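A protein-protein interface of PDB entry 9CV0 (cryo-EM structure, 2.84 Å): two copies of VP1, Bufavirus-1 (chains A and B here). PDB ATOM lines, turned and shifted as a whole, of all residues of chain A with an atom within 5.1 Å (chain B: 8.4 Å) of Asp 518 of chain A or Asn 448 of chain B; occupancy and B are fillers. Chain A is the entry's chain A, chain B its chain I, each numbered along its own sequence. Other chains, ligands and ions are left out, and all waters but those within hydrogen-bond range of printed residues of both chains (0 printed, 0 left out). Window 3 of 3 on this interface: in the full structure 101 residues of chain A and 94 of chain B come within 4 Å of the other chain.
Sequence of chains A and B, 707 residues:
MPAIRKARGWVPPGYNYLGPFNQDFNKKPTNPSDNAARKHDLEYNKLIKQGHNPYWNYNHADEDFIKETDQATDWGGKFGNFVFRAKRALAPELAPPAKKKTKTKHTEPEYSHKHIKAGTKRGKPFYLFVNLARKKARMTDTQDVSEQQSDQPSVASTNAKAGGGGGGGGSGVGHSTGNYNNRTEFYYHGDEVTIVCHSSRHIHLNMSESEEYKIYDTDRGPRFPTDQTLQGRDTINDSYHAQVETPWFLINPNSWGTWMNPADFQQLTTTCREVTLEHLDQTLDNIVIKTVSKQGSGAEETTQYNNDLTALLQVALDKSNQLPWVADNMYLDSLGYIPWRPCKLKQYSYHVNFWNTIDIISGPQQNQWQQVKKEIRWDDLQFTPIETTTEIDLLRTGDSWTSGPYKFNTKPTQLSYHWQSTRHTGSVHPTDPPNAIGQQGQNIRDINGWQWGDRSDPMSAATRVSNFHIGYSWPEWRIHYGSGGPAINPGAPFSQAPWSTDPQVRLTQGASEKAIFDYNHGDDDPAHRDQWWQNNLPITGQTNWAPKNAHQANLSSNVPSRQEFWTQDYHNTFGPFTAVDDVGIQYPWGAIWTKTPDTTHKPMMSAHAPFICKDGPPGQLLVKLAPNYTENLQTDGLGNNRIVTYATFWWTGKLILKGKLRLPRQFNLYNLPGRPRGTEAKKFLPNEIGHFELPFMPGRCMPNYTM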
ATOM      1  N   TYR A 331       7.562 -17.370  25.858  1.00  0.00           N
ATOM      2  CA  TYR A 331       7.019 -18.463  25.003  1.00  0.00           C
ATOM      3  C   TYR A 331       7.853 -18.498  23.717  1.00  0.00           C
ATOM      4  O   TYR A 331       7.463 -19.210  22.778  1.00  0.00           O
ATOM      5  CB  TYR A 331       5.512 -18.299  24.793  1.00  0.00           C
ATOM      6  CG  TYR A 331       4.707 -18.368  26.065  1.00  0.00           C
ATOM      7  CD1 TYR A 331       4.868 -19.418  26.953  1.00  0.00           C
ATOM      8  CD2 TYR A 331       3.784 -17.387  26.385  1.00  0.00           C
ATOM      9  CE1 TYR A 331       4.137 -19.492  28.126  1.00  0.00           C
ATOM     10  CE2 TYR A 331       3.043 -17.447  27.552  1.00  0.00           C
ATOM     11  CZ  TYR A 331       3.219 -18.502  28.427  1.00  0.00           C
ATOM     12  OH  TYR A 331       2.493 -18.568  29.580  1.00  0.00           O
ATOM     13  N   LEU A 332       8.971 -17.768  23.694  1.00  0.00           N
ATOM     14  CA  LEU A 332       9.909 -17.758  22.535  1.00  0.00           C
ATOM     15  C   LEU A 332       9.175 -17.921  21.203  1.00  0.00           C
ATOM     16  O   LEU A 332       9.617 -18.757  20.396  1.00  0.00           O
ATOM     17  CB  LEU A 332      10.958 -18.860  22.733  1.00  0.00           C
ATOM     18  CG  LEU A 332      12.251 -18.416  23.416  1.00  0.00           C
ATOM     19  CD1 LEU A 332      11.958 -17.609  24.670  1.00  0.00           C
ATOM     20  CD2 LEU A 332      13.131 -19.609  23.742  1.00  0.00           C
ATOM     21  N   ASP A 333       8.113 -17.149  20.975  1.00  0.00           N
ATOM     22  CA  ASP A 333       7.456 -17.191  19.677  1.00  0.00           C
ATOM     23  C   ASP A 333       7.974 -15.961  18.957  1.00  0.00           C
ATOM     24  O   ASP A 333       7.509 -14.845  19.173  1.00  0.00           O
ATOM     25  CB  ASP A 333       5.940 -17.184  19.819  1.00  0.00           C
ATOM     26  CG  ASP A 333       5.398 -18.469  20.426  1.00  0.00           C
ATOM     27  OD1 ASP A 333       6.118 -19.489  20.428  1.00  0.00           O
ATOM     28  OD2 ASP A 333       4.251 -18.455  20.917  1.00  0.00           O
ATOM     29  N   ILE A 516      13.907 -22.001  27.752  1.00  0.00           N
ATOM     30  CA  ILE A 516      13.650 -23.300  27.152  1.00  0.00           C
ATOM     31  C   ILE A 516      13.383 -23.020  25.683  1.00  0.00           C
ATOM     32  O   ILE A 516      12.496 -22.233  25.351  1.00  0.00           O
ATOM     33  CB  ILE A 516      12.475 -24.015  27.822  1.00  0.00           C
ATOM     34  CG1 ILE A 516      12.811 -24.319  29.280  1.00  0.00           C
ATOM     35  CG2 ILE A 516      12.139 -25.283  27.080  1.00  0.00           C
ATOM     36  CD1 ILE A 516      12.280 -23.306  30.252  1.00  0.00           C
ATOM     37  N   PHE A 517      14.171 -23.617  24.799  1.00  0.00           N
ATOM     38  CA  PHE A 517      14.180 -23.241  23.393  1.00  0.00           C
ATOM     39  C   PHE A 517      14.256 -24.478  22.515  1.00  0.00           C
ATOM     40  O   PHE A 517      14.362 -25.605  22.995  1.00  0.00           O
ATOM     41  CB  PHE A 517      15.339 -22.279  23.102  1.00  0.00           C
ATOM     42  CG  PHE A 517      16.665 -22.760  23.600  1.00  0.00           C
ATOM     43  CD1 PHE A 517      17.496 -23.515  22.797  1.00  0.00           C
ATOM     44  CD2 PHE A 517      17.075 -22.467  24.883  1.00  0.00           C
ATOM     45  CE1 PHE A 517      18.704 -23.956  23.262  1.00  0.00           C
ATOM     46  CE2 PHE A 517      18.279 -22.910  25.348  1.00  0.00           C
ATOM     47  CZ  PHE A 517      19.095 -23.656  24.535  1.00  0.00           C
ATOM     48  N   ASP A 518      14.202 -24.259  21.208  1.00  0.00           N
ATOM     49  CA  ASP A 518      13.970 -25.353  20.276  1.00  0.00           C
ATOM     50  C   ASP A 518      14.863 -25.142  19.058  1.00  0.00           C
ATOM     51  O   ASP A 518      15.696 -24.233  19.015  1.00  0.00           O
ATOM     52  CB  ASP A 518      12.477 -25.438  19.934  1.00  0.00           C
ATOM     53  CG  ASP A 518      12.103 -26.753  19.296  1.00  0.00           C
ATOM     54  OD1 ASP A 518      12.975 -27.644  19.228  1.00  0.00           O
ATOM     55  OD2 ASP A 518      10.939 -26.897  18.863  1.00  0.00           O
ATOM     56  N   TYR A 519      14.671 -25.992  18.049  1.00  0.00           N
ATOM     57  CA  TYR A 519      15.622 -26.132  16.951  1.00  0.00           C
ATOM     58  C   TYR A 519      15.833 -24.819  16.207  1.00  0.00           C
ATOM     59  O   TYR A 519      16.967 -24.448  15.890  1.00  0.00           O
ATOM     60  CB  TYR A 519      15.118 -27.226  16.014  1.00  0.00           C
ATOM     61  CG  TYR A 519      15.944 -27.476  14.786  1.00  0.00           C
ATOM     62  CD1 TYR A 519      17.144 -28.163  14.863  1.00  0.00           C
ATOM     63  CD2 TYR A 519      15.501 -27.071  13.541  1.00  0.00           C
ATOM     64  CE1 TYR A 519      17.887 -28.411  13.745  1.00  0.00           C
ATOM     65  CE2 TYR A 519      16.241 -27.313  12.417  1.00  0.00           C
ATOM     66  CZ  TYR A 519      17.432 -27.984  12.523  1.00  0.00           C
ATOM     67  OH  TYR A 519      18.173 -28.233  11.397  1.00  0.00           O
ATOM     68  N   ASN A 520      14.748 -24.103  15.918  1.00  0.00           N
ATOM     69  CA  ASN A 520      14.845 -22.846  15.190  1.00  0.00           C
ATOM     70  C   ASN A 520      15.417 -21.729  16.056  1.00  0.00           C
ATOM     71  O   ASN A 520      16.009 -20.782  15.529  1.00  0.00           O
ATOM     72  CB  ASN A 520      13.459 -22.465  14.669  1.00  0.00           C
ATOM     73  CG  ASN A 520      13.502 -21.420  13.576  1.00  0.00           C
ATOM     74  OD1 ASN A 520      14.435 -21.372  12.775  1.00  0.00           O
ATOM     75  ND2 ASN A 520      12.479 -20.574  13.535  1.00  0.00           N
ATOM     76  N   HIS A 521      15.242 -21.827  17.370  1.00  0.00           N
ATOM     77  CA  HIS A 521      15.685 -20.832  18.338  1.00  0.00           C
ATOM     78  C   HIS A 521      17.032 -21.171  18.967  1.00  0.00           C
ATOM     79  O   HIS A 521      17.366 -20.656  20.035  1.00  0.00           O
ATOM     80  CB  HIS A 521      14.599 -20.590  19.381  1.00  0.00           C
ATOM     81  CG  HIS A 521      13.427 -19.840  18.831  1.00  0.00           C
ATOM     82  ND1 HIS A 521      12.397 -20.456  18.157  1.00  0.00           N
ATOM     83  CD2 HIS A 521      13.157 -18.515  18.797  1.00  0.00           C
ATOM     84  CE1 HIS A 521      11.527 -19.546  17.760  1.00  0.00           C
ATOM     85  NE2 HIS A 521      11.965 -18.359  18.137  1.00  0.00           N
ATOM     86  N   GLY A 522      17.788 -22.076  18.355  1.00  0.00           N
ATOM     87  CA  GLY A 522      19.154 -22.289  18.794  1.00  0.00           C
ATOM     88  C   GLY A 522      19.425 -23.572  19.537  1.00  0.00           C
ATOM     89  O   GLY A 522      20.440 -23.677  20.228  1.00  0.00           O
ATOM     90  N   ASP A 523      18.523 -24.539  19.449  1.00  0.00           N
ATOM     91  CA  ASP A 523      18.769 -25.898  19.897  1.00  0.00           C
ATOM     92  C   ASP A 523      19.286 -26.711  18.723  1.00  0.00           C
ATOM     93  O   ASP A 523      18.861 -26.516  17.583  1.00  0.00           O
ATOM     94  CB  ASP A 523      17.497 -26.533  20.445  1.00  0.00           C
ATOM     95  CG  ASP A 523      17.714 -27.927  20.966  1.00  0.00           C
ATOM     96  OD1 ASP A 523      18.874 -28.366  21.076  1.00  0.00           O
ATOM     97  OD2 ASP A 523      16.709 -28.603  21.241  1.00  0.00           O
ATOM     98  N   ASP A 525      19.129 -30.158  18.603  1.00  0.00           N
ATOM     99  CA  ASP A 525      18.378 -31.389  18.426  1.00  0.00           C
ATOM    100  C   ASP A 525      16.957 -31.068  17.989  1.00  0.00           C
ATOM    101  O   ASP A 525      16.256 -30.342  18.705  1.00  0.00           O
ATOM    102  CB  ASP A 525      18.362 -32.181  19.729  1.00  0.00           C
ATOM    103  CG  ASP A 525      17.777 -33.562  19.564  1.00  0.00           C
ATOM    104  OD1 ASP A 525      17.533 -33.970  18.414  1.00  0.00           O
ATOM    105  OD2 ASP A 525      17.553 -34.240  20.586  1.00  0.00           O
ATOM    106  N   ALA A 527      13.067 -32.371  17.672  1.00  0.00           N
ATOM    107  CA  ALA A 527      12.178 -33.227  18.445  1.00  0.00           C
ATOM    108  C   ALA A 527      12.491 -33.200  19.939  1.00  0.00           C
ATOM    109  O   ALA A 527      11.768 -33.827  20.711  1.00  0.00           O
ATOM    110  CB  ALA A 527      12.170 -34.693  17.966  1.00  0.00           C
ATOM    111  N   HIS A 528      13.542 -32.512  20.374  1.00  0.00           N
ATOM    112  CA  HIS A 528      13.795 -32.291  21.788  1.00  0.00           C
ATOM    113  C   HIS A 528      14.188 -30.837  21.980  1.00  0.00           C
ATOM    114  O   HIS A 528      14.605 -30.169  21.034  1.00  0.00           O
ATOM    115  CB  HIS A 528      14.880 -33.223  22.325  1.00  0.00           C
ATOM    116  CG  HIS A 528      14.487 -34.667  22.312  1.00  0.00           C
ATOM    117  ND1 HIS A 528      14.568 -35.450  21.182  1.00  0.00           N
ATOM    118  CD2 HIS A 528      14.001 -35.468  23.290  1.00  0.00           C
ATOM    119  CE1 HIS A 528      14.154 -36.672  21.464  1.00  0.00           C
ATOM    120  NE2 HIS A 528      13.803 -36.709  22.736  1.00  0.00           N
ATOM    121  N   ARG A 529      14.029 -30.346  23.203  1.00  0.00           N
ATOM    122  CA  ARG A 529      14.302 -28.955  23.532  1.00  0.00           C
ATOM    123  C   ARG A 529      15.464 -28.861  24.503  1.00  0.00           C
ATOM    124  O   ARG A 529      15.639 -29.737  25.354  1.00  0.00           O
ATOM    125  CB  ARG A 529      13.072 -28.276  24.125  1.00  0.00           C
ATOM    126  CG  ARG A 529      12.021 -27.981  23.107  1.00  0.00           C
ATOM    127  CD  ARG A 529      10.821 -27.322  23.723  1.00  0.00           C
ATOM    128  NE  ARG A 529       9.854 -26.950  22.698  1.00  0.00           N
ATOM    129  CZ  ARG A 529       8.965 -27.782  22.174  1.00  0.00           C
ATOM    130  NH1 ARG A 529       8.917 -29.043  22.575  1.00  0.00           N
ATOM    131  NH2 ARG A 529       8.124 -27.353  21.248  1.00  0.00           N
ATOM    132  N   SER B 427       1.978 -12.143  26.201  1.00  0.00           N
ATOM    133  CA  SER B 427       1.717 -13.309  25.380  1.00  0.00           C
ATOM    134  C   SER B 427       0.939 -14.350  26.166  1.00  0.00           C
ATOM    135  O   SER B 427       1.102 -14.502  27.376  1.00  0.00           O
ATOM    136  CB  SER B 427       3.029 -13.903  24.873  1.00  0.00           C
ATOM    137  OG  SER B 427       3.843 -14.319  25.948  1.00  0.00           O
ATOM    138  N   HIS B 429      -0.457 -18.183  27.068  1.00  0.00           N
ATOM    139  CA  HIS B 429       0.106 -19.519  27.134  1.00  0.00           C
ATOM    140  C   HIS B 429      -0.334 -20.307  25.906  1.00  0.00           C
ATOM    141  O   HIS B 429      -1.510 -20.239  25.527  1.00  0.00           O
ATOM    142  CB  HIS B 429      -0.358 -20.233  28.400  1.00  0.00           C
ATOM    143  CG  HIS B 429       0.376 -21.503  28.681  1.00  0.00           C
ATOM    144  ND1 HIS B 429       1.671 -21.523  29.145  1.00  0.00           N
ATOM    145  CD2 HIS B 429       0.020 -22.796  28.516  1.00  0.00           C
ATOM    146  CE1 HIS B 429       2.065 -22.772  29.292  1.00  0.00           C
ATOM    147  NE2 HIS B 429       1.085 -23.565  28.909  1.00  0.00           N
ATOM    148  N   PRO B 430       0.563 -21.035  25.246  1.00  0.00           N
ATOM    149  CA  PRO B 430       0.140 -21.840  24.096  1.00  0.00           C
ATOM    150  C   PRO B 430      -0.989 -22.791  24.444  1.00  0.00           C
ATOM    151  O   PRO B 430      -0.915 -23.532  25.426  1.00  0.00           O
ATOM    152  CB  PRO B 430       1.419 -22.584  23.712  1.00  0.00           C
ATOM    153  CG  PRO B 430       2.499 -21.677  24.158  1.00  0.00           C
ATOM    154  CD  PRO B 430       2.022 -21.073  25.427  1.00  0.00           C
ATOM    155  N   ILE B 444      -0.849 -26.474  26.118  1.00  0.00           N
ATOM    156  CA  ILE B 444       0.111 -27.397  25.533  1.00  0.00           C
ATOM    157  C   ILE B 444       1.225 -27.670  26.530  1.00  0.00           C
ATOM    158  O   ILE B 444       1.733 -26.760  27.195  1.00  0.00           O
ATOM    159  CB  ILE B 444       0.655 -26.825  24.214  1.00  0.00           C
ATOM    160  CG1 ILE B 444      -0.477 -26.676  23.207  1.00  0.00           C
ATOM    161  CG2 ILE B 444       1.721 -27.723  23.643  1.00  0.00           C
ATOM    162  CD1 ILE B 444      -0.089 -25.921  21.985  1.00  0.00           C
ATOM    163  N   ARG B 445       1.607 -28.940  26.643  1.00  0.00           N
ATOM    164  CA  ARG B 445       2.539 -29.393  27.669  1.00  0.00           C
ATOM    165  C   ARG B 445       3.983 -29.030  27.334  1.00  0.00           C
ATOM    166  O   ARG B 445       4.635 -28.307  28.092  1.00  0.00           O
ATOM    167  CB  ARG B 445       2.377 -30.899  27.881  1.00  0.00           C
ATOM    168  CG  ARG B 445       1.010 -31.254  28.424  1.00  0.00           C
ATOM    169  CD  ARG B 445       0.860 -32.741  28.644  1.00  0.00           C
ATOM    170  NE  ARG B 445      -0.465 -33.091  29.149  1.00  0.00           N
ATOM    171  CZ  ARG B 445      -0.881 -34.337  29.353  1.00  0.00           C
ATOM    172  NH1 ARG B 445      -2.103 -34.566  29.814  1.00  0.00           N
ATOM    173  NH2 ARG B 445      -0.073 -35.358  29.098  1.00  0.00           N
ATOM    174  N   ASP B 446       4.503 -29.529  26.216  1.00  0.00           N
ATOM    175  CA  ASP B 446       5.884 -29.232  25.839  1.00  0.00           C
ATOM    176  C   ASP B 446       5.885 -27.985  24.969  1.00  0.00           C
ATOM    177  O   ASP B 446       5.490 -27.988  23.802  1.00  0.00           O
ATOM    178  CB  ASP B 446       6.518 -30.412  25.117  1.00  0.00           C
ATOM    179  CG  ASP B 446       6.823 -31.569  26.042  1.00  0.00           C
ATOM    180  OD1 ASP B 446       6.895 -31.354  27.269  1.00  0.00           O
ATOM    181  OD2 ASP B 446       6.976 -32.702  25.540  1.00  0.00           O
ATOM    182  N   ILE B 447       6.376 -26.907  25.550  1.00  0.00           N
ATOM    183  CA  ILE B 447       6.506 -25.637  24.875  1.00  0.00           C
ATOM    184  C   ILE B 447       7.841 -25.041  25.276  1.00  0.00           C
ATOM    185  O   ILE B 447       8.506 -25.496  26.207  1.00  0.00           O
ATOM    186  CB  ILE B 447       5.358 -24.657  25.203  1.00  0.00           C
ATOM    187  CG1 ILE B 447       5.304 -24.397  26.702  1.00  0.00           C
ATOM    188  CG2 ILE B 447       4.028 -25.168  24.687  1.00  0.00           C
ATOM    189  CD1 ILE B 447       4.445 -23.261  27.058  1.00  0.00           C
ATOM    190  N   ASN B 448       8.236 -23.997  24.569  1.00  0.00           N
ATOM    191  CA  ASN B 448       9.490 -23.323  24.833  1.00  0.00           C
ATOM    192  C   ASN B 448       9.234 -21.877  25.238  1.00  0.00           C
ATOM    193  O   ASN B 448       8.321 -21.229  24.731  1.00  0.00           O
ATOM    194  CB  ASN B 448      10.403 -23.404  23.603  1.00  0.00           C
ATOM    195  CG  ASN B 448       9.797 -22.777  22.378  1.00  0.00           C
ATOM    196  OD1 ASN B 448       8.606 -22.490  22.341  1.00  0.00           O
ATOM    197  ND2 ASN B 448      10.612 -22.574  21.356  1.00  0.00           N
ATOM    198  N   GLY B 449      10.021 -21.389  26.187  1.00  0.00           N
ATOM    199  CA  GLY B 449       9.903 -20.010  26.613  1.00  0.00           C
ATOM    200  C   GLY B 449      10.726 -19.733  27.849  1.00  0.00           C
ATOM    201  O   GLY B 449      11.417 -20.599  28.378  1.00  0.00           O
ATOM    202  N   TRP B 450      10.621 -18.492  28.307  1.00  0.00           N
ATOM    203  CA  TRP B 450      11.319 -18.022  29.496  1.00  0.00           C
ATOM    204  C   TRP B 450      10.483 -18.227  30.753  1.00  0.00           C
ATOM    205  O   TRP B 450       9.411 -17.639  30.886  1.00  0.00           O
ATOM    206  CB  TRP B 450      11.640 -16.538  29.365  1.00  0.00           C
ATOM    207  CG  TRP B 450      12.745 -16.136  28.494  1.00  0.00           C
ATOM    208  CD1 TRP B 450      12.664 -15.725  27.212  1.00  0.00           C
ATOM    209  CD2 TRP B 450      14.115 -16.035  28.864  1.00  0.00           C
ATOM    210  NE1 TRP B 450      13.902 -15.404  26.740  1.00  0.00           N
ATOM    211  CE2 TRP B 450      14.815 -15.584  27.742  1.00  0.00           C
ATOM    212  CE3 TRP B 450      14.823 -16.298  30.037  1.00  0.00           C
ATOM    213  CZ2 TRP B 450      16.186 -15.387  27.752  1.00  0.00           C
ATOM    214  CZ3 TRP B 450      16.180 -16.105  30.040  1.00  0.00           C
ATOM    215  CH2 TRP B 450      16.847 -15.657  28.908  1.00  0.00           C
ATOM    216  N   GLN B 451      10.994 -19.026  31.688  1.00  0.00           N
ATOM    217  CA  GLN B 451      10.433 -19.219  33.018  1.00  0.00           C
ATOM    218  C   GLN B 451      11.280 -18.420  34.015  1.00  0.00           C
ATOM    219  O   GLN B 451      12.208 -17.710  33.598  1.00  0.00           O
ATOM    220  CB  GLN B 451      10.362 -20.715  33.306  1.00  0.00           C
ATOM    221  CG  GLN B 451       9.404 -21.465  32.400  1.00  0.00           C
ATOM    222  CD  GLN B 451       7.962 -21.103  32.630  1.00  0.00           C
ATOM    223  OE1 GLN B 451       7.489 -21.114  33.757  1.00  0.00           O
ATOM    224  NE2 GLN B 451       7.264 -20.731  31.568  1.00  0.00           N
ATOM    225  N   SER B 456      11.621 -25.812  33.765  1.00  0.00           N
ATOM    226  CA  SER B 456      11.765 -26.011  32.298  1.00  0.00           C
ATOM    227  C   SER B 456      10.594 -26.870  31.823  1.00  0.00           C
ATOM    228  O   SER B 456      10.095 -26.623  30.716  1.00  0.00           O
ATOM    229  CB  SER B 456      13.084 -26.642  31.980  1.00  0.00           C
ATOM    230  OG  SER B 456      13.282 -27.814  32.756  1.00  0.00           O
ATOM    231  N   MET B 459       6.392 -24.993  33.011  1.00  0.00           N
ATOM    232  CA  MET B 459       6.112 -23.869  32.076  1.00  0.00           C
ATOM    233  C   MET B 459       4.752 -23.269  32.451  1.00  0.00           C
ATOM    234  O   MET B 459       4.072 -22.748  31.544  1.00  0.00           O
ATOM    235  CB  MET B 459       6.053 -24.347  30.623  1.00  0.00           C
ATOM    236  CG  MET B 459       7.266 -25.157  30.203  1.00  0.00           C
ATOM    237  SD  MET B 459       8.795 -24.187  30.219  1.00  0.00           S
ATOM    238  CE  MET B 459       8.433 -22.982  28.942  1.00  0.00           C
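The backbone carbonyl oxygen (O) of Tyr 331 of chain A sits close to the backbone carbonyl oxygen (O) of Asn 448 of chain B (2.9 Å). The side-chain hydroxyl of Tyr 331 of chain A lies within hydrogen-bond range of a ring nitrogen (ND1) of His 429 of chain B (3.1 Å). The backbone NH (N) of Gly 449 of chain B lies within hydrogen-bond range of the backbone carbonyl oxygen (O) of Ile 516 of chain A (2.7 Å).
The backbone carbonyl oxygen of Tyr 331 of chain A sits close to the side-chain carboxylate of Asp 333 of chain A, 2.7 Å away. The guanidinium group (NH2) of Arg 529 of chain A lies within salt-bridge range of the side-chain carboxylate (OD2) of Asp 518 of chain A (3.7 Å). O of Asp 518 of chain A lies within hydrogen-bond range of N of Asp 523 of chain A (2.9 Å). O of Pro 430 of chain B is in hydrogen-bond range of N of Ile 444 of chain B, 3.0 Å away. NE2 of His 521 of chain A lies within hydrogen-bond range of O of Leu 332 of chain A, at 3.3 Å.
Pro 430 of chain B touches Tyr 331 of chain A (CD to CD1, 3.6 Å). Leu 332 of chain A touches Asn 448 of chain B. Gly 449 of chain B touches Leu 332 of chain A. Leu 332 of chain A touches Trp 450 of chain B (CD1 to CD1, 3.2 Å). Ile 447 of chain B touches Ile 516 of chain A (O to CG2, 3.7 Å). Ile 516 of chain A touches Asn 448 of chain B (O to CB, 3.0 Å). CA of Phe 517 of chain A touches CB of Asn 448 of chain B, 3.8 Å away. CB of Asp 518 of chain A touches ND2 of Asn 448 of chain B, 3.7 Å away. Arg 529 of chain A touches Asp 446 of chain B. Arg 529 of chain A touches Asn 448 of chain B (NE to CB, 3.7 Å).
No position is printed for both chains. Of the 19 pairs that touch across the chains among the printed residues, none has its exchanged pair printed and touching as well.
Asp 518 of chain A touches just one residue of chain B: Asn 448 (3.7 Å). Of chain A, only Tyr 331, Leu 332, Ile 516, Phe 517, Asp 518 and Arg 529 come within 4 Å of Asn 448 of chain B. Printed residues of chain A within 4 Å of Ile 447 of chain B: Tyr 331, Ile 516 and Arg 529. Printed residues of chain A within 4 Å of Asp 446 of chain B: Arg 529 (3.7 Å). The nearest printed residue of chain B that does not touch Asp 518 of chain A is Ile 447 of chain B (7.1 Å).
Hydrophobic or aromatic side chains of chain A that line the printed part of chain B: Tyr 331, Leu 332 and Ile 516. Of the 13 printed residues of chain B, 10 touch a printed residue of chain A. Printed residues of chain B that touch a printed residue of chain A: Ser 427, His 429, Pro 430, Asp 446, Ile 447, Asn 448, Gly 449, Trp 450, Ser 456 and Met 459. Hydrophobic or aromatic side chains of chain B within 4 Å of the printed part of chain A: His 429, Pro 430, Ile 447, Trp 450 and Met 459. Among the printed residues, 19 pairs touch across the chains. Among the printed residues, no Asp or Glu carboxylate lies within 4 Å of a Lys or Arg side-chain nitrogen of the other chain.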
